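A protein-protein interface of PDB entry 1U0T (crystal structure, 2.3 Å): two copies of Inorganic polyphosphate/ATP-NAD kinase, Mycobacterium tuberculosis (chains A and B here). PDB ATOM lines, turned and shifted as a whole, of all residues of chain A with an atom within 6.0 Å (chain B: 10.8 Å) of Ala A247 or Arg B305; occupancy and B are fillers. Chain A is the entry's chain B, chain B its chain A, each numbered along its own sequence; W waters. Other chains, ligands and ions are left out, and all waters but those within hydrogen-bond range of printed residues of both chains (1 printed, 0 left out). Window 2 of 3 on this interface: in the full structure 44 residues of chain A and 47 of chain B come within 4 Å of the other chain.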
ATOM      1  N   VAL A 175      -9.165  -0.558  -1.771  1.00  0.00           N
ATOM      2  CA  VAL A 175      -8.086   0.181  -2.400  1.00  0.00           C
ATOM      3  C   VAL A 175      -7.055  -0.892  -2.793  1.00  0.00           C
ATOM      4  O   VAL A 175      -6.663  -1.691  -1.934  1.00  0.00           O
ATOM      5  CB  VAL A 175      -7.403   1.184  -1.414  1.00  0.00           C
ATOM      6  CG1 VAL A 175      -6.323   1.924  -2.105  1.00  0.00           C
ATOM      7  CG2 VAL A 175      -8.428   2.200  -0.829  1.00  0.00           C
ATOM      8  N   GLU A 177      -3.225  -1.641  -3.914  1.00  0.00           N
ATOM      9  CA  GLU A 177      -1.982  -0.976  -3.678  1.00  0.00           C
ATOM     10  C   GLU A 177      -0.906  -1.878  -4.279  1.00  0.00           C
ATOM     11  O   GLU A 177      -0.901  -3.101  -4.032  1.00  0.00           O
ATOM     12  CB  GLU A 177      -1.769  -0.782  -2.177  1.00  0.00           C
ATOM     13  CG  GLU A 177      -0.338  -0.443  -1.772  1.00  0.00           C
ATOM     14  CD  GLU A 177      -0.089  -0.671  -0.286  1.00  0.00           C
ATOM     15  OE1 GLU A 177      -0.746   0.002   0.567  1.00  0.00           O
ATOM     16  OE2 GLU A 177       0.770  -1.519   0.028  1.00  0.00           O
ATOM     17  N   GLU A 244      -6.685  -3.161   0.464  1.00  0.00           N
ATOM     18  CA  GLU A 244      -7.442  -2.672   1.639  1.00  0.00           C
ATOM     19  C   GLU A 244      -8.972  -2.775   1.510  1.00  0.00           C
ATOM     20  O   GLU A 244      -9.532  -2.388   0.516  1.00  0.00           O
ATOM     21  CB  GLU A 244      -7.061  -1.215   1.981  1.00  0.00           C
ATOM     22  CG  GLU A 244      -5.578  -1.037   2.373  1.00  0.00           C
ATOM     23  CD  GLU A 244      -5.155   0.445   2.473  1.00  0.00           C
ATOM     24  OE1 GLU A 244      -4.055   0.735   2.985  1.00  0.00           O
ATOM     25  OE2 GLU A 244      -5.918   1.340   2.064  1.00  0.00           O
ATOM     26  N   ILE A 245      -9.612  -3.296   2.551  1.00  0.00           N
ATOM     27  CA  ILE A 245     -11.058  -3.540   2.631  1.00  0.00           C
ATOM     28  C   ILE A 245     -11.645  -2.394   3.454  1.00  0.00           C
ATOM     29  O   ILE A 245     -11.128  -2.116   4.552  1.00  0.00           O
ATOM     30  CB  ILE A 245     -11.311  -4.853   3.437  1.00  0.00           C
ATOM     31  CG1 ILE A 245     -10.401  -6.008   2.970  1.00  0.00           C
ATOM     32  CG2 ILE A 245     -12.805  -5.212   3.514  1.00  0.00           C
ATOM     33  CD1 ILE A 245     -10.267  -6.200   1.492  1.00  0.00           C
ATOM     34  N   GLU A 246     -12.713  -1.751   2.953  1.00  0.00           N
ATOM     35  CA  GLU A 246     -13.264  -0.563   3.625  1.00  0.00           C
ATOM     36  C   GLU A 246     -13.568  -0.837   5.113  1.00  0.00           C
ATOM     37  O   GLU A 246     -14.140  -1.890   5.461  1.00  0.00           O
ATOM     38  CB  GLU A 246     -14.496  -0.024   2.906  1.00  0.00           C
ATOM     39  CG  GLU A 246     -15.801  -0.670   3.335  1.00  0.00           C
ATOM     40  CD  GLU A 246     -16.685  -1.032   2.150  1.00  0.00           C
ATOM     41  OE1 GLU A 246     -16.819  -2.265   1.799  1.00  0.00           O
ATOM     42  OE2 GLU A 246     -17.232  -0.055   1.581  1.00  0.00           O
ATOM     43  N   ALA A 247     -13.146   0.104   5.968  1.00  0.00           N
ATOM     44  CA  ALA A 247     -13.343   0.019   7.423  1.00  0.00           C
ATOM     45  C   ALA A 247     -14.815   0.018   7.825  1.00  0.00           C
ATOM     46  O   ALA A 247     -15.225  -0.680   8.759  1.00  0.00           O
ATOM     47  CB  ALA A 247     -12.591   1.158   8.145  1.00  0.00           C
ATOM     48  N   ASP A 248     -15.614   0.774   7.102  1.00  0.00           N
ATOM     49  CA  ASP A 248     -17.009   0.939   7.481  1.00  0.00           C
ATOM     50  C   ASP A 248     -17.938  -0.240   7.110  1.00  0.00           C
ATOM     51  O   ASP A 248     -18.966  -0.440   7.767  1.00  0.00           O
ATOM     52  CB  ASP A 248     -17.556   2.280   6.945  1.00  0.00           C
ATOM     53  CG  ASP A 248     -18.211   2.150   5.547  1.00  0.00           C
ATOM     54  OD1 ASP A 248     -18.017   3.054   4.690  1.00  0.00           O
ATOM     55  OD2 ASP A 248     -18.973   1.203   5.223  1.00  0.00           O
ATOM     56  N   GLY A 249     -17.562  -1.017   6.093  1.00  0.00           N
ATOM     57  CA  GLY A 249     -18.436  -2.021   5.503  1.00  0.00           C
ATOM     58  C   GLY A 249     -18.387  -3.398   6.139  1.00  0.00           C
ATOM     59  O   GLY A 249     -17.939  -3.564   7.276  1.00  0.00           O
ATOM     60  N   ALA A 266     -13.515  -6.439   7.974  1.00  0.00           N
ATOM     61  CA  ALA A 266     -13.579  -5.049   7.533  1.00  0.00           C
ATOM     62  C   ALA A 266     -12.389  -4.262   8.110  1.00  0.00           C
ATOM     63  O   ALA A 266     -11.989  -4.479   9.258  1.00  0.00           O
ATOM     64  CB  ALA A 266     -14.924  -4.411   7.976  1.00  0.00           C
ATOM     65  N   GLY A 267     -11.806  -3.372   7.312  1.00  0.00           N
ATOM     66  CA  GLY A 267     -10.690  -2.592   7.776  1.00  0.00           C
ATOM     67  C   GLY A 267      -9.371  -3.349   7.778  1.00  0.00           C
ATOM     68  O   GLY A 267      -8.334  -2.766   7.986  1.00  0.00           O
ATOM     69  N   SER A 268      -9.405  -4.647   7.527  1.00  0.00           N
ATOM     70  CA  SER A 268      -8.162  -5.368   7.388  1.00  0.00           C
ATOM     71  C   SER A 268      -7.518  -5.159   6.006  1.00  0.00           C
ATOM     72  O   SER A 268      -7.976  -4.349   5.189  1.00  0.00           O
ATOM     73  CB  SER A 268      -8.372  -6.862   7.658  1.00  0.00           C
ATOM     74  OG  SER A 268      -8.743  -7.504   6.456  1.00  0.00           O
ATOM     75  N   ARG A 269      -6.453  -5.913   5.761  1.00  0.00           N
ATOM     76  CA  ARG A 269      -5.675  -5.736   4.556  1.00  0.00           C
ATOM     77  C   ARG A 269      -5.002  -7.042   4.147  1.00  0.00           C
ATOM     78  O   ARG A 269      -4.396  -7.743   4.982  1.00  0.00           O
ATOM     79  CB  ARG A 269      -4.683  -4.607   4.787  1.00  0.00           C
ATOM     80  CG  ARG A 269      -3.275  -4.830   4.290  1.00  0.00           C
ATOM     81  CD  ARG A 269      -2.366  -3.625   4.581  1.00  0.00           C
ATOM     82  NE  ARG A 269      -1.055  -3.730   3.954  1.00  0.00           N
ATOM     83  CZ  ARG A 269      -0.608  -2.853   3.049  1.00  0.00           C
ATOM     84  NH1 ARG A 269      -1.394  -1.843   2.684  1.00  0.00           N
ATOM     85  NH2 ARG A 269       0.600  -2.989   2.496  1.00  0.00           N
ATOM     86  N   VAL B 301      -7.799   7.468  -5.924  1.00  0.00           N
ATOM     87  CA  VAL B 301      -7.048   6.729  -4.910  1.00  0.00           C
ATOM     88  C   VAL B 301      -7.391   7.126  -3.450  1.00  0.00           C
ATOM     89  O   VAL B 301      -6.624   6.846  -2.507  1.00  0.00           O
ATOM     90  CB  VAL B 301      -5.535   6.829  -5.213  1.00  0.00           C
ATOM     91  CG1 VAL B 301      -4.744   6.609  -4.000  1.00  0.00           C
ATOM     92  CG2 VAL B 301      -5.101   5.797  -6.339  1.00  0.00           C
ATOM     93  N   THR B 302      -8.554   7.748  -3.255  1.00  0.00           N
ATOM     94  CA  THR B 302      -8.880   8.254  -1.935  1.00  0.00           C
ATOM     95  C   THR B 302      -9.369   7.114  -1.068  1.00  0.00           C
ATOM     96  O   THR B 302     -10.059   6.211  -1.549  1.00  0.00           O
ATOM     97  CB  THR B 302      -9.925   9.403  -2.014  1.00  0.00           C
ATOM     98  OG1 THR B 302     -10.981   9.004  -2.890  1.00  0.00           O
ATOM     99  CG2 THR B 302      -9.342  10.649  -2.714  1.00  0.00           C
ATOM    100  N   GLY B 303      -9.009   7.174   0.212  1.00  0.00           N
ATOM    101  CA  GLY B 303      -9.303   6.125   1.178  1.00  0.00           C
ATOM    102  C   GLY B 303      -8.089   5.272   1.564  1.00  0.00           C
ATOM    103  O   GLY B 303      -8.180   4.456   2.484  1.00  0.00           O
ATOM    104  N   TRP B 304      -6.969   5.444   0.855  1.00  0.00           N
ATOM    105  CA  TRP B 304      -5.755   4.646   1.068  1.00  0.00           C
ATOM    106  C   TRP B 304      -5.236   4.792   2.492  1.00  0.00           C
ATOM    107  O   TRP B 304      -4.947   5.899   2.914  1.00  0.00           O
ATOM    108  CB  TRP B 304      -4.632   5.099   0.106  1.00  0.00           C
ATOM    109  CG  TRP B 304      -3.368   4.280   0.225  1.00  0.00           C
ATOM    110  CD1 TRP B 304      -3.277   2.921   0.202  1.00  0.00           C
ATOM    111  CD2 TRP B 304      -2.037   4.763   0.409  1.00  0.00           C
ATOM    112  NE1 TRP B 304      -1.970   2.523   0.323  1.00  0.00           N
ATOM    113  CE2 TRP B 304      -1.187   3.636   0.475  1.00  0.00           C
ATOM    114  CE3 TRP B 304      -1.466   6.043   0.527  1.00  0.00           C
ATOM    115  CZ2 TRP B 304       0.203   3.742   0.643  1.00  0.00           C
ATOM    116  CZ3 TRP B 304      -0.101   6.149   0.693  1.00  0.00           C
ATOM    117  CH2 TRP B 304       0.724   5.005   0.760  1.00  0.00           C
ATOM    118  N   ARG B 305      -5.068   3.678   3.201  1.00  0.00           N
ATOM    119  CA  ARG B 305      -4.436   3.712   4.532  1.00  0.00           C
ATOM    120  C   ARG B 305      -2.910   3.577   4.499  1.00  0.00           C
ATOM    121  O   ARG B 305      -2.208   4.425   5.081  1.00  0.00           O
ATOM    122  CB  ARG B 305      -5.083   2.702   5.484  1.00  0.00           C
ATOM    123  CG  ARG B 305      -6.550   3.040   5.750  1.00  0.00           C
ATOM    124  CD  ARG B 305      -7.320   2.045   6.626  1.00  0.00           C
ATOM    125  NE  ARG B 305      -7.374   0.655   6.155  1.00  0.00           N
ATOM    126  CZ  ARG B 305      -8.463   0.042   5.649  1.00  0.00           C
ATOM    127  NH1 ARG B 305      -9.589   0.697   5.465  1.00  0.00           N
ATOM    128  NH2 ARG B 305      -8.418  -1.246   5.302  1.00  0.00           N
ATOM    129  N   GLY B 306      -2.420   2.534   3.808  1.00  0.00           N
ATOM    130  CA  GLY B 306      -1.000   2.210   3.669  1.00  0.00           C
ATOM    131  C   GLY B 306      -0.431   1.330   4.774  1.00  0.00           C
ATOM    132  O   GLY B 306      -1.151   0.970   5.708  1.00  0.00           O
HETATM  133  O   HOH W   1      -8.261   1.933   2.396  1.00  0.00           O
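NH2 of Arg B305 is in hydrogen-bond range of O of Ile A245. N of Gly B306 is in hydrogen-bond range of OE1 of Glu A244, 2.6 Å away. The guanidinium group of Arg B305 sits at hydrogen-bond distance from the backbone carbonyl oxygen of Gly A267, 3.1 Å away. The side-chain carboxylate (OE1) of Glu A177 sits at hydrogen-bond distance from the indole nitrogen (NE1) of Trp B304, 2.8 Å away. The guanidinium group (NH2) of Arg B305 lies within hydrogen-bond range of the backbone carbonyl oxygen (O) of Ser A268 (3.1 Å). The backbone NH (N) of Arg B305 is in hydrogen-bond range of the side-chain carboxylate (OE2) of Glu A244.
O of Ile A245 is in hydrogen-bond range of N of Gly A267 (3.1 Å). O of Glu A246 is in hydrogen-bond range of N of Gly A267. The guanidinium group (NH1) of Arg A269 lies within salt-bridge range of the side-chain carboxylate (OE1) of Glu A244, at 3.7 Å. NH2 of Arg A269 is in salt-bridge range of OE2 of Glu A177, 2.9 Å away. The backbone carbonyl oxygen (O) of Ser A268 lies within hydrogen-bond range of the backbone NH (N) of Ile A245 (3.3 Å). O of Val A175 lies within hydrogen-bond range of N of Glu A244, at 2.8 Å.
Val A175 touches Gly B303. N of Trp B304 touches CG2 of Val A175 (3.9 Å). Gly B306 touches Glu A177 (CA to OE1, 3.8 Å). Glu A244 touches Gly B303 (OE2 to O, 3.9 Å). Trp B304 touches Glu A244. Ala A247 touches Arg B305 (N to NH1, 3.6 Å). Gly B306 touches Arg A269.
Printed residues of chain B within 4 Å of Glu A177: Trp B304 (2.8 Å) and Gly B306 (3.8 Å). Of chain B, only Gly B303 (3.9 Å), Trp B304 (3.5 Å), Arg B305 (2.7 Å) and Gly B306 (2.6 Å) come within 4 Å of Glu A244. No residue of chain B comes within 4 Å of Glu A246. Of chain B, only Arg B305 (3.6 Å) comes within 4 Å of Ala A247. No residue of chain B comes within 4 Å of Asp A248. No residue of chain B comes within 4 Å of Gly A249. Of chain B, only Arg B305 (3.1 Å) comes within 4 Å of Gly A267. Ser A268 touches just one residue of chain B: Arg B305. Val B301 touches none of the printed residues of chain A. Thr B302 touches none of the printed residues of chain A. Of the printed residues of chain A, Gly B303 touches Val A175 (3.9 Å) and Glu A244 (3.9 Å). Of chain A, only Glu A244, Ile A245, Ala A247, Gly A267 and Ser A268 come within 4 Å of Arg B305.
Of the 6 printed residues of chain B, 4 touch a printed residue of chain A. Hydrophobic or aromatic side chains of chain B within 4 Å of the printed part of chain A: Trp B304. Of the 12 printed residues of chain A, 8 touch a printed residue of chain B. Printed residues of chain A that touch a printed residue of chain B: Val A175, Glu A177, Glu A244, Ile A245, Ala A247, Gly A267, Ser A268 and Arg A269. Hydrophobic or aromatic side chains of chain A that line the printed part of chain B: Val A175. Among the printed residues, no Asp or Glu carboxylate lies within 4 Å of a Lys or Arg side-chain nitrogen of the other chain.
No position is printed for both chains. Of the 13 pairs that touch across the chains among the printed residues, none has its exchanged pair printed and touching as well.
Water W1 lies within hydrogen-bond range of the side-chain carboxylate of Glu A244 (2.4 Å) and the backbone carbonyl oxygen of Gly B303 (2.5 Å).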
